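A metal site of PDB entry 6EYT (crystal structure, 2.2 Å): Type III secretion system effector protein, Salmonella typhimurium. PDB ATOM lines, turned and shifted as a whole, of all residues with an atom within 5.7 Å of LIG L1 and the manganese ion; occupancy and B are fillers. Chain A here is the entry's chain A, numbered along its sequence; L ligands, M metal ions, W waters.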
ATOM      1  N   PHE A  42      12.068 -12.246 -26.164  1.00  0.00           N
ATOM      2  CA  PHE A  42      13.439 -11.810 -26.035  1.00  0.00           C
ATOM      3  C   PHE A  42      14.259 -12.970 -25.504  1.00  0.00           C
ATOM      4  O   PHE A  42      13.717 -13.889 -24.889  1.00  0.00           O
ATOM      5  CB  PHE A  42      13.558 -10.595 -25.117  1.00  0.00           C
ATOM      6  CG  PHE A  42      12.849  -9.379 -25.634  1.00  0.00           C
ATOM      7  CD1 PHE A  42      13.458  -8.542 -26.565  1.00  0.00           C
ATOM      8  CD2 PHE A  42      11.564  -9.076 -25.211  1.00  0.00           C
ATOM      9  CE1 PHE A  42      12.802  -7.424 -27.059  1.00  0.00           C
ATOM     10  CE2 PHE A  42      10.899  -7.959 -25.700  1.00  0.00           C
ATOM     11  CZ  PHE A  42      11.514  -7.127 -26.620  1.00  0.00           C
ATOM     12  N   GLN A  43      15.566 -12.927 -25.767  1.00  0.00           N
ATOM     13  CA  GLN A  43      16.474 -13.978 -25.332  1.00  0.00           C
ATOM     14  C   GLN A  43      17.692 -13.357 -24.656  1.00  0.00           C
ATOM     15  O   GLN A  43      18.282 -12.403 -25.177  1.00  0.00           O
ATOM     16  CB  GLN A  43      16.931 -14.831 -26.523  1.00  0.00           C
ATOM     17  CG  GLN A  43      17.889 -15.954 -26.144  1.00  0.00           C
ATOM     18  CD  GLN A  43      18.456 -16.627 -27.366  1.00  0.00           C
ATOM     19  OE1 GLN A  43      18.574 -16.003 -28.417  1.00  0.00           O
ATOM     20  NE2 GLN A  43      18.804 -17.909 -27.237  1.00  0.00           N
ATOM     21  N   TRP A  44      18.070 -13.891 -23.502  1.00  0.00           N
ATOM     22  CA  TRP A  44      19.333 -13.483 -22.875  1.00  0.00           C
ATOM     23  C   TRP A  44      20.005 -14.721 -22.298  1.00  0.00           C
ATOM     24  O   TRP A  44      19.628 -15.197 -21.225  1.00  0.00           O
ATOM     25  CB  TRP A  44      19.137 -12.420 -21.811  1.00  0.00           C
ATOM     26  CG  TRP A  44      20.468 -11.936 -21.362  1.00  0.00           C
ATOM     27  CD1 TRP A  44      21.058 -12.165 -20.149  1.00  0.00           C
ATOM     28  CD2 TRP A  44      21.418 -11.208 -22.144  1.00  0.00           C
ATOM     29  NE1 TRP A  44      22.314 -11.600 -20.127  1.00  0.00           N
ATOM     30  CE2 TRP A  44      22.562 -11.010 -21.340  1.00  0.00           C
ATOM     31  CE3 TRP A  44      21.418 -10.703 -23.444  1.00  0.00           C
ATOM     32  CZ2 TRP A  44      23.681 -10.308 -21.792  1.00  0.00           C
ATOM     33  CZ3 TRP A  44      22.527 -10.015 -23.897  1.00  0.00           C
ATOM     34  CH2 TRP A  44      23.649  -9.825 -23.070  1.00  0.00           C
ATOM     35  N   PHE A  45      21.004 -15.238 -23.026  1.00  0.00           N
ATOM     36  CA  PHE A  45      21.869 -16.305 -22.543  1.00  0.00           C
ATOM     37  C   PHE A  45      23.131 -15.700 -21.947  1.00  0.00           C
ATOM     38  O   PHE A  45      23.912 -15.058 -22.659  1.00  0.00           O
ATOM     39  CB  PHE A  45      22.231 -17.273 -23.680  1.00  0.00           C
ATOM     40  CG  PHE A  45      21.139 -18.238 -24.029  1.00  0.00           C
ATOM     41  CD1 PHE A  45      19.809 -17.923 -23.756  1.00  0.00           C
ATOM     42  CD2 PHE A  45      21.433 -19.454 -24.607  1.00  0.00           C
ATOM     43  CE1 PHE A  45      18.791 -18.823 -24.070  1.00  0.00           C
ATOM     44  CE2 PHE A  45      20.430 -20.359 -24.913  1.00  0.00           C
ATOM     45  CZ  PHE A  45      19.107 -20.034 -24.648  1.00  0.00           C
ATOM     46  N   GLU A  46      23.336 -15.903 -20.654  1.00  0.00           N
ATOM     47  CA  GLU A  46      24.462 -15.318 -19.948  1.00  0.00           C
ATOM     48  C   GLU A  46      25.483 -16.414 -19.665  1.00  0.00           C
ATOM     49  O   GLU A  46      25.201 -17.362 -18.917  1.00  0.00           O
ATOM     50  CB  GLU A  46      24.014 -14.670 -18.634  1.00  0.00           C
ATOM     51  CG  GLU A  46      25.147 -14.071 -17.833  1.00  0.00           C
ATOM     52  CD  GLU A  46      25.945 -13.054 -18.639  1.00  0.00           C
ATOM     53  OE1 GLU A  46      25.322 -12.108 -19.150  1.00  0.00           O
ATOM     54  OE2 GLU A  46      27.171 -13.221 -18.787  1.00  0.00           O
ATOM     55  N   ARG A  47      26.676 -16.294 -20.244  1.00  0.00           N
ATOM     56  CA  ARG A  47      27.698 -17.299 -20.014  1.00  0.00           C
ATOM     57  C   ARG A  47      28.578 -16.973 -18.805  1.00  0.00           C
ATOM     58  O   ARG A  47      29.348 -17.837 -18.389  1.00  0.00           O
ATOM     59  CB  ARG A  47      28.560 -17.519 -21.254  1.00  0.00           C
ATOM     60  CG  ARG A  47      28.893 -16.307 -22.095  1.00  0.00           C
ATOM     61  CD  ARG A  47      29.461 -16.835 -23.406  1.00  0.00           C
ATOM     62  NE  ARG A  47      30.054 -15.796 -24.247  1.00  0.00           N
ATOM     63  CZ  ARG A  47      29.363 -14.982 -25.021  1.00  0.00           C
ATOM     64  NH1 ARG A  47      28.037 -15.059 -25.062  1.00  0.00           N
ATOM     65  NH2 ARG A  47      29.990 -14.075 -25.769  1.00  0.00           N
ATOM     66  N   ARG A  51      29.151 -11.949 -13.297  1.00  0.00           N
ATOM     67  CA  ARG A  51      29.445 -10.547 -13.533  1.00  0.00           C
ATOM     68  C   ARG A  51      28.309  -9.635 -13.071  1.00  0.00           C
ATOM     69  O   ARG A  51      28.495  -8.410 -13.045  1.00  0.00           O
ATOM     70  CB  ARG A  51      29.743 -10.289 -15.013  1.00  0.00           C
ATOM     71  CG  ARG A  51      28.539 -10.302 -15.958  1.00  0.00           C
ATOM     72  CD  ARG A  51      29.024 -10.395 -17.399  1.00  0.00           C
ATOM     73  NE  ARG A  51      27.963 -10.520 -18.395  1.00  0.00           N
ATOM     74  CZ  ARG A  51      27.729  -9.630 -19.359  1.00  0.00           C
ATOM     75  NH1 ARG A  51      28.490  -8.559 -19.488  1.00  0.00           N
ATOM     76  NH2 ARG A  51      26.727  -9.832 -20.215  1.00  0.00           N
ATOM     77  N   ASN A  65      24.427  -1.059 -23.645  1.00  0.00           N
ATOM     78  CA  ASN A  65      23.492  -2.104 -24.030  1.00  0.00           C
ATOM     79  C   ASN A  65      22.393  -2.188 -22.980  1.00  0.00           C
ATOM     80  O   ASN A  65      22.422  -3.064 -22.106  1.00  0.00           O
ATOM     81  CB  ASN A  65      24.200  -3.451 -24.199  1.00  0.00           C
ATOM     82  CG  ASN A  65      25.243  -3.430 -25.291  1.00  0.00           C
ATOM     83  OD1 ASN A  65      26.427  -3.207 -25.040  1.00  0.00           O
ATOM     84  ND2 ASN A  65      24.813  -3.670 -26.529  1.00  0.00           N
ATOM     85  N   TYR A  67      19.590  -3.495 -22.436  1.00  0.00           N
ATOM     86  CA  TYR A  67      18.658  -4.484 -22.976  1.00  0.00           C
ATOM     87  C   TYR A  67      17.528  -4.788 -22.001  1.00  0.00           C
ATOM     88  O   TYR A  67      16.365  -4.918 -22.408  1.00  0.00           O
ATOM     89  CB  TYR A  67      19.421  -5.758 -23.350  1.00  0.00           C
ATOM     90  CG  TYR A  67      20.323  -5.547 -24.544  1.00  0.00           C
ATOM     91  CD1 TYR A  67      20.412  -4.310 -25.161  1.00  0.00           C
ATOM     92  CD2 TYR A  67      21.096  -6.588 -25.039  1.00  0.00           C
ATOM     93  CE1 TYR A  67      21.248  -4.104 -26.257  1.00  0.00           C
ATOM     94  CE2 TYR A  67      21.933  -6.403 -26.137  1.00  0.00           C
ATOM     95  CZ  TYR A  67      22.008  -5.152 -26.732  1.00  0.00           C
ATOM     96  OH  TYR A  67      22.828  -4.956 -27.816  1.00  0.00           O
ATOM     97  N   PHE A 182      23.262 -19.822 -28.429  1.00  0.00           N
ATOM     98  CA  PHE A 182      21.959 -19.202 -28.270  1.00  0.00           C
ATOM     99  C   PHE A 182      21.244 -19.015 -29.601  1.00  0.00           C
ATOM    100  O   PHE A 182      20.010 -19.010 -29.634  1.00  0.00           O
ATOM    101  CB  PHE A 182      22.032 -17.894 -27.457  1.00  0.00           C
ATOM    102  CG  PHE A 182      22.941 -16.832 -28.001  1.00  0.00           C
ATOM    103  CD1 PHE A 182      22.557 -16.044 -29.081  1.00  0.00           C
ATOM    104  CD2 PHE A 182      24.114 -16.507 -27.325  1.00  0.00           C
ATOM    105  CE1 PHE A 182      23.379 -15.015 -29.530  1.00  0.00           C
ATOM    106  CE2 PHE A 182      24.929 -15.488 -27.766  1.00  0.00           C
ATOM    107  CZ  PHE A 182      24.570 -14.736 -28.874  1.00  0.00           C
ATOM    108  N   ARG A 186      17.461 -20.490 -30.054  1.00  0.00           N
ATOM    109  CA  ARG A 186      16.451 -19.553 -30.549  1.00  0.00           C
ATOM    110  C   ARG A 186      15.573 -20.233 -31.588  1.00  0.00           C
ATOM    111  O   ARG A 186      14.347 -20.105 -31.551  1.00  0.00           O
ATOM    112  CB  ARG A 186      17.127 -18.313 -31.129  1.00  0.00           C
ATOM    113  CG  ARG A 186      16.169 -17.226 -31.642  1.00  0.00           C
ATOM    114  CD  ARG A 186      16.944 -16.075 -32.268  1.00  0.00           C
ATOM    115  NE  ARG A 186      17.932 -15.534 -31.337  1.00  0.00           N
ATOM    116  CZ  ARG A 186      18.907 -14.703 -31.686  1.00  0.00           C
ATOM    117  NH1 ARG A 186      19.033 -14.292 -32.946  1.00  0.00           N
ATOM    118  NH2 ARG A 186      19.760 -14.265 -30.761  1.00  0.00           N
ATOM    119  N   TYR A 216      10.091 -13.220 -32.302  1.00  0.00           N
ATOM    120  CA  TYR A 216      11.374 -13.044 -31.637  1.00  0.00           C
ATOM    121  C   TYR A 216      12.020 -11.729 -32.041  1.00  0.00           C
ATOM    122  O   TYR A 216      12.023 -11.366 -33.220  1.00  0.00           O
ATOM    123  CB  TYR A 216      12.349 -14.185 -31.945  1.00  0.00           C
ATOM    124  CG  TYR A 216      13.710 -13.798 -31.451  1.00  0.00           C
ATOM    125  CD1 TYR A 216      14.049 -13.964 -30.122  1.00  0.00           C
ATOM    126  CD2 TYR A 216      14.633 -13.187 -32.298  1.00  0.00           C
ATOM    127  CE1 TYR A 216      15.283 -13.571 -29.640  1.00  0.00           C
ATOM    128  CE2 TYR A 216      15.865 -12.784 -31.819  1.00  0.00           C
ATOM    129  CZ  TYR A 216      16.186 -12.988 -30.490  1.00  0.00           C
ATOM    130  OH  TYR A 216      17.405 -12.591 -30.016  1.00  0.00           O
ATOM    131  N   LEU A 217      12.614 -11.038 -31.071  1.00  0.00           N
ATOM    132  CA  LEU A 217      13.264  -9.768 -31.328  1.00  0.00           C
ATOM    133  C   LEU A 217      14.563  -9.714 -30.556  1.00  0.00           C
ATOM    134  O   LEU A 217      14.615 -10.122 -29.389  1.00  0.00           O
ATOM    135  CB  LEU A 217      12.390  -8.568 -30.924  1.00  0.00           C
ATOM    136  CG  LEU A 217      11.060  -8.279 -31.630  1.00  0.00           C
ATOM    137  CD1 LEU A 217      10.374  -7.150 -30.917  1.00  0.00           C
ATOM    138  CD2 LEU A 217      11.253  -7.937 -33.106  1.00  0.00           C
ATOM    139  N   ASP A 218      15.610  -9.206 -31.195  1.00  0.00           N
ATOM    140  CA  ASP A 218      16.822  -8.893 -30.458  1.00  0.00           C
ATOM    141  C   ASP A 218      16.513  -7.801 -29.445  1.00  0.00           C
ATOM    142  O   ASP A 218      15.705  -6.895 -29.714  1.00  0.00           O
ATOM    143  CB  ASP A 218      17.935  -8.457 -31.416  1.00  0.00           C
ATOM    144  CG  ASP A 218      18.775  -9.610 -31.910  1.00  0.00           C
ATOM    145  OD1 ASP A 218      18.553 -10.751 -31.448  1.00  0.00           O
ATOM    146  OD2 ASP A 218      19.652  -9.391 -32.783  1.00  0.00           O
ATOM    147  N   ALA A 219      17.135  -7.884 -28.276  1.00  0.00           N
ATOM    148  CA  ALA A 219      16.807  -6.932 -27.215  1.00  0.00           C
ATOM    149  C   ALA A 219      17.146  -5.511 -27.617  1.00  0.00           C
ATOM    150  O   ALA A 219      16.673  -4.566 -26.963  1.00  0.00           O
ATOM    151  CB  ALA A 219      17.526  -7.318 -25.923  1.00  0.00           C
ATOM    152  N   ASP A 220      17.951  -5.316 -28.661  1.00  0.00           N
ATOM    153  CA  ASP A 220      18.233  -3.979 -29.166  1.00  0.00           C
ATOM    154  C   ASP A 220      17.270  -3.550 -30.276  1.00  0.00           C
ATOM    155  O   ASP A 220      17.483  -2.482 -30.878  1.00  0.00           O
ATOM    156  CB  ASP A 220      19.683  -3.895 -29.666  1.00  0.00           C
ATOM    157  CG  ASP A 220      19.890  -4.649 -30.978  1.00  0.00           C
ATOM    158  OD1 ASP A 220      18.947  -5.291 -31.484  1.00  0.00           O
ATOM    159  OD2 ASP A 220      21.017  -4.601 -31.498  1.00  0.00           O
ATOM    160  N   ASP A 317      18.185  -3.146 -34.638  1.00  0.00           N
ATOM    161  CA  ASP A 317      19.613  -3.374 -34.393  1.00  0.00           C
ATOM    162  C   ASP A 317      20.324  -2.116 -33.889  1.00  0.00           C
ATOM    163  O   ASP A 317      21.317  -1.654 -34.463  1.00  0.00           O
ATOM    164  CB  ASP A 317      20.303  -3.918 -35.652  1.00  0.00           C
ATOM    165  CG  ASP A 317      21.742  -4.412 -35.397  1.00  0.00           C
ATOM    166  OD1 ASP A 317      22.068  -4.752 -34.241  1.00  0.00           O
ATOM    167  OD2 ASP A 317      22.538  -4.483 -36.351  1.00  0.00           O
ATOM    168  N   THR A 318      19.820  -1.577 -32.782  1.00  0.00           N
ATOM    169  CA  THR A 318      20.433  -0.393 -32.194  1.00  0.00           C
ATOM    170  C   THR A 318      21.812  -0.650 -31.592  1.00  0.00           C
ATOM    171  O   THR A 318      22.539   0.321 -31.324  1.00  0.00           O
ATOM    172  CB  THR A 318      19.528   0.208 -31.110  1.00  0.00           C
ATOM    173  OG1 THR A 318      19.280  -0.777 -30.091  1.00  0.00           O
ATOM    174  CG2 THR A 318      18.222   0.691 -31.716  1.00  0.00           C
ATOM    175  N   SER A 319      22.214  -1.912 -31.411  1.00  0.00           N
ATOM    176  CA  SER A 319      23.560  -2.170 -30.911  1.00  0.00           C
ATOM    177  C   SER A 319      24.604  -1.703 -31.916  1.00  0.00           C
ATOM    178  O   SER A 319      25.711  -1.309 -31.524  1.00  0.00           O
ATOM    179  CB  SER A 319      23.756  -3.657 -30.630  1.00  0.00           C
ATOM    180  OG  SER A 319      23.722  -4.406 -31.840  1.00  0.00           O
ATOM    181  N   SER A 320      24.270  -1.742 -33.212  1.00  0.00           N
ATOM    182  CA  SER A 320      25.189  -1.255 -34.222  1.00  0.00           C
ATOM    183  C   SER A 320      25.471   0.239 -34.064  1.00  0.00           C
ATOM    184  O   SER A 320      26.466   0.725 -34.603  1.00  0.00           O
ATOM    185  CB  SER A 320      24.624  -1.548 -35.605  1.00  0.00           C
ATOM    186  OG  SER A 320      23.438  -0.811 -35.824  1.00  0.00           O
ATOM    187  N   ILE A 323      27.779  -0.676 -29.485  1.00  0.00           N
ATOM    188  CA  ILE A 323      28.683  -1.830 -29.560  1.00  0.00           C
ATOM    189  C   ILE A 323      27.847  -3.074 -29.370  1.00  0.00           C
ATOM    190  O   ILE A 323      26.848  -3.070 -28.644  1.00  0.00           O
ATOM    191  CB  ILE A 323      29.811  -1.753 -28.498  1.00  0.00           C
ATOM    192  CG1 ILE A 323      29.206  -1.592 -27.088  1.00  0.00           C
ATOM    193  CG2 ILE A 323      30.822  -0.664 -28.827  1.00  0.00           C
ATOM    194  CD1 ILE A 323      30.216  -1.770 -25.981  1.00  0.00           C
ATOM    195  N   SER A 324      28.250  -4.153 -30.042  1.00  0.00           N
ATOM    196  CA  SER A 324      27.633  -5.458 -29.817  1.00  0.00           C
ATOM    197  C   SER A 324      27.834  -5.879 -28.365  1.00  0.00           C
ATOM    198  O   SER A 324      28.806  -5.493 -27.707  1.00  0.00           O
ATOM    199  CB  SER A 324      28.224  -6.503 -30.752  1.00  0.00           C
ATOM    200  OG  SER A 324      27.844  -7.822 -30.368  1.00  0.00           O
ATOM    201  N   SER A 325      26.882  -6.658 -27.850  1.00  0.00           N
ATOM    202  CA  SER A 325      27.038  -7.180 -26.499  1.00  0.00           C
ATOM    203  C   SER A 325      27.924  -8.421 -26.435  1.00  0.00           C
ATOM    204  O   SER A 325      28.318  -8.818 -25.338  1.00  0.00           O
ATOM    205  CB  SER A 325      25.663  -7.488 -25.881  1.00  0.00           C
ATOM    206  OG  SER A 325      24.910  -8.356 -26.708  1.00  0.00           O
ATOM    207  N   TRP A 326      28.264  -9.030 -27.586  1.00  0.00           N
ATOM    208  CA  TRP A 326      29.063 -10.254 -27.566  1.00  0.00           C
ATOM    209  C   TRP A 326      30.199 -10.292 -28.587  1.00  0.00           C
ATOM    210  O   TRP A 326      31.072 -11.166 -28.463  1.00  0.00           O
ATOM    211  CB  TRP A 326      28.168 -11.478 -27.805  1.00  0.00           C
ATOM    212  CG  TRP A 326      27.535 -11.491 -29.147  1.00  0.00           C
ATOM    213  CD1 TRP A 326      26.364 -10.878 -29.514  1.00  0.00           C
ATOM    214  CD2 TRP A 326      28.016 -12.156 -30.316  1.00  0.00           C
ATOM    215  NE1 TRP A 326      26.093 -11.131 -30.843  1.00  0.00           N
ATOM    216  CE2 TRP A 326      27.105 -11.907 -31.354  1.00  0.00           C
ATOM    217  CE3 TRP A 326      29.147 -12.935 -30.580  1.00  0.00           C
ATOM    218  CZ2 TRP A 326      27.277 -12.419 -32.634  1.00  0.00           C
ATOM    219  CZ3 TRP A 326      29.321 -13.434 -31.855  1.00  0.00           C
ATOM    220  CH2 TRP A 326      28.389 -13.180 -32.864  1.00  0.00           C
ATOM    221  N   ARG A 327      30.224  -9.414 -29.588  1.00  0.00           N
ATOM    222  CA  ARG A 327      31.320  -9.427 -30.569  1.00  0.00           C
ATOM    223  C   ARG A 327      32.541  -8.662 -30.076  1.00  0.00           C
ATOM    224  O   ARG A 327      32.441  -7.800 -29.192  1.00  0.00           O
ATOM    225  CB  ARG A 327      30.863  -8.839 -31.915  1.00  0.00           C
ATOM    226  CG  ARG A 327      29.683  -9.571 -32.532  1.00  0.00           C
ATOM    227  CD  ARG A 327      29.224  -8.882 -33.806  1.00  0.00           C
ATOM    228  NE  ARG A 327      27.942  -9.405 -34.280  1.00  0.00           N
ATOM    229  CZ  ARG A 327      27.818 -10.344 -35.217  1.00  0.00           C
ATOM    230  NH1 ARG A 327      28.908 -10.857 -35.783  1.00  0.00           N
ATOM    231  NH2 ARG A 327      26.625 -10.763 -35.586  1.00  0.00           N
HETATM  232  N1  LIG L   1      22.706 -12.437 -26.681  1.00  0.00           N
HETATM  233  C1  LIG L   1      22.628 -13.265 -25.589  1.00  0.00           C
HETATM  234  N2  LIG L   1      23.707 -13.223 -24.748  1.00  0.00           N
HETATM  235  C2  LIG L   1      24.845 -12.451 -24.890  1.00  0.00           C
HETATM  236  C3  LIG L   1      24.852 -11.609 -26.042  1.00  0.00           C
HETATM  237  C4  LIG L   1      23.801 -11.634 -26.890  1.00  0.00           C
HETATM  238  O1  LIG L   1      21.674 -13.993 -25.365  1.00  0.00           O
HETATM  239  O2  LIG L   1      25.744 -12.517 -24.034  1.00  0.00           O
HETATM  240  C5  LIG L   1      21.570 -12.429 -27.616  1.00  0.00           C
HETATM  241  C6  LIG L   1      20.426 -11.517 -27.150  1.00  0.00           C
HETATM  242  O3  LIG L   1      19.182 -12.111 -27.479  1.00  0.00           O
HETATM  243  C7  LIG L   1      20.650 -10.262 -28.003  1.00  0.00           C
HETATM  244  C8  LIG L   1      21.143 -10.873 -29.306  1.00  0.00           C
HETATM  245  O4  LIG L   1      22.009 -11.958 -28.874  1.00  0.00           O
HETATM  246  O5  LIG L   1      19.439  -9.553 -28.188  1.00  0.00           O
HETATM  247  C9  LIG L   1      21.903  -9.946 -30.220  1.00  0.00           C
HETATM  248  O6  LIG L   1      22.709  -9.050 -29.414  1.00  0.00           O
HETATM  249  P1  LIG L   1      23.469  -7.821 -30.057  1.00  0.00           P
HETATM  250  O7  LIG L   1      22.455  -7.033 -30.821  1.00  0.00           O
HETATM  251  O8  LIG L   1      24.288  -7.064 -29.006  1.00  0.00           O
HETATM  252  O9  LIG L   1      24.525  -8.474 -31.060  1.00  0.00           O
HETATM  253  P2  LIG L   1      24.665  -8.186 -32.619  1.00  0.00           P
HETATM  254  O10 LIG L   1      23.550  -7.371 -33.134  1.00  0.00           O
HETATM  255  O11 LIG L   1      24.725  -9.595 -33.229  1.00  0.00           O
HETATM  256  O12 LIG L   1      26.032  -7.525 -32.718  1.00  0.00           O
HETATM  257  C1  LG2 L   2      23.130 -11.287 -35.999  1.00  0.00           C
HETATM  258  C2  LG2 L   2      21.810 -11.145 -35.198  1.00  0.00           C
HETATM  259  C3  LG2 L   2      21.948 -11.761 -33.785  1.00  0.00           C
HETATM  260  C4  LG2 L   2      22.555 -13.169 -33.898  1.00  0.00           C
HETATM  261  C5  LG2 L   2      23.925 -13.059 -34.576  1.00  0.00           C
HETATM  262  C6  LG2 L   2      24.677 -14.386 -34.690  1.00  0.00           C
HETATM  263  C7  LG2 L   2      20.674  -9.149 -36.193  1.00  0.00           C
HETATM  264  C8  LG2 L   2      20.363  -7.659 -36.035  1.00  0.00           C
HETATM  265  O1  LG2 L   2      23.690 -12.609 -35.923  1.00  0.00           O
HETATM  266  O2  LG2 L   2      20.681 -11.834 -33.141  1.00  0.00           O
HETATM  267  O3  LG2 L   2      22.640 -13.763 -32.603  1.00  0.00           O
HETATM  268  O4  LG2 L   2      24.073 -15.263 -35.653  1.00  0.00           O
HETATM  269  O5  LG2 L   2      20.279  -9.766 -37.192  1.00  0.00           O
HETATM  270  N1  LG2 L   2      21.401  -9.741 -35.184  1.00  0.00           N
HETATM  271  O6  LG2 L   2      24.044 -10.328 -35.532  1.00  0.00           O
HETATM  272 MN    MN M   1      22.364  -5.895 -32.523  1.00  0.00          MN
HETATM  273  O   HOH W   1      20.271  -7.305 -29.215  1.00  0.00           O
HETATM  274  O   HOH W   2      26.855 -13.600 -21.847  1.00  0.00           O
HETATM  275  O   HOH W   3      24.556  -5.898 -35.603  1.00  0.00           O
HETATM  276  O   HOH W   4      20.379  -6.756 -33.280  1.00  0.00           O
HETATM  277  O   HOH W   5      16.475 -10.926 -27.527  1.00  0.00           O
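Water W4 lies within hydrogen-bond range of the side-chain carboxylate of Asp 220 (2.7 Å) and the side-chain carboxylate of Asp 218 (2.8 Å). Water W1 lies within hydrogen-bond range of O5 of LIG L1 (2.6 Å), N of Asp 220 (3.1 Å) and N of Ala 219 (3.3 Å). Water W5 lies within hydrogen-bond range of O of Leu 217 (2.8 Å), N of Gln 43 (2.8 Å), O3 of LIG L1 (3.0 Å), OH of Tyr 216 (3.1 Å) and N of Ala 219 (3.2 Å).
An oxygen (O6) of LG2 L2 is in hydrogen-bond range of an oxygen (O11) of LIG L1, at 2.5 Å.
O of Asp 317 sits at hydrogen-bond distance from OG of Ser 320, at 2.7 Å. The backbone carbonyl oxygen (O) of Asp 220 lies within hydrogen-bond range of the side-chain hydroxyl (OG1) of Thr 318, 2.6 Å away. NE2 of Gln 43 sits at hydrogen-bond distance from O of Phe 182, at 2.9 Å. NE of Arg 186 is in hydrogen-bond range of OE1 of Gln 43, 3.0 Å away. The side-chain amide nitrogen (ND2) of Asn 65 is in hydrogen-bond range of the side-chain hydroxyl (OH) of Tyr 67, at 2.7 Å. The side-chain hydroxyl of Tyr 216 sits at hydrogen-bond distance from the side-chain carboxylate of Asp 218 (2.6 Å). The side-chain hydroxyl (OH) of Tyr 216 is in hydrogen-bond range of the guanidinium group (NH2) of Arg 186 (3.0 Å). The indole nitrogen (NE1) of Trp 44 is in hydrogen-bond range of the side-chain carboxylate (OE1) of Glu 46, 3.2 Å away.
Three residues have an atom within 4 Å of the manganese ion: Asp 220, Asp 317 and Ser 319.
The backbone carbonyl oxygen (O) of Gln 43 sits at hydrogen-bond distance from an oxygen (O3) of LIG L1. O8 of LIG L1 is in hydrogen-bond range of N of Ser 325, 2.9 Å away. OG of Ser 325 is in hydrogen-bond range of O8 of LIG L1 (2.7 Å). An oxygen (O1) of LIG L1 sits at hydrogen-bond distance from the backbone NH (N) of Phe 45, 2.7 Å away. A nitrogen (N2) of LIG L1 lies within hydrogen-bond range of the backbone carbonyl oxygen (O) of Phe 45 (2.8 Å). The side-chain hydroxyl (OH) of Tyr 67 is in hydrogen-bond range of an oxygen (O8) of LIG L1 (2.8 Å). An oxygen (O5) of LIG L1 is in hydrogen-bond range of the backbone NH (N) of Ala 219 (2.8 Å). The side-chain hydroxyl (OG) of Ser 324 is in hydrogen-bond range of an oxygen (O12) of LIG L1 (3.0 Å). The indole nitrogen (NE1) of Trp 326 is in hydrogen-bond range of an oxygen (O9) of LIG L1, 3.1 Å away. An oxygen (O12) of LIG L1 lies within salt-bridge range of the guanidinium group of Arg 327. OH of Tyr 216 lies within hydrogen-bond range of O3 of LIG L1 (3.1 Å). NH2 of Arg 327 lies within hydrogen-bond range of O6 of LG2 L2 (2.6 Å). OD2 of Asp 218 is in hydrogen-bond range of O2 of LG2 L2. An oxygen (O2) of LG2 L2 lies within hydrogen-bond range of the guanidinium group (NH1) of Arg 186 (3.0 Å).
An oxygen (O10) of LIG L1 is bound to the manganese ion. The manganese ion is bound by an oxygen (O7) of LIG L1 (2.0 Å). OD1 of Asp 317 binds the manganese ion, at 2.1 Å. OG of Ser 319 is bound to the manganese ion (2.1 Å). OD2 of Asp 220 binds the manganese ion (2.1 Å). Water W4 is bound to the manganese ion (2.3 Å).
Residues that only touch LIG L1: Asp 218 (3.4 Å), Trp 44 (3.4 Å), Phe 182 (3.4 Å), Arg 47 (3.6 Å) and Arg 186 (3.7 Å). Hydrophobic or aromatic side chains that line LIG L1: Trp 44, Phe 45, Tyr 67, Phe 182, Ala 219 and Trp 326. Of the 25 residues printed, 17 come within 4 Å of LIG L1. The nearest printed residue that does not touch LIG L1 is Asn 65 (4.2 Å).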
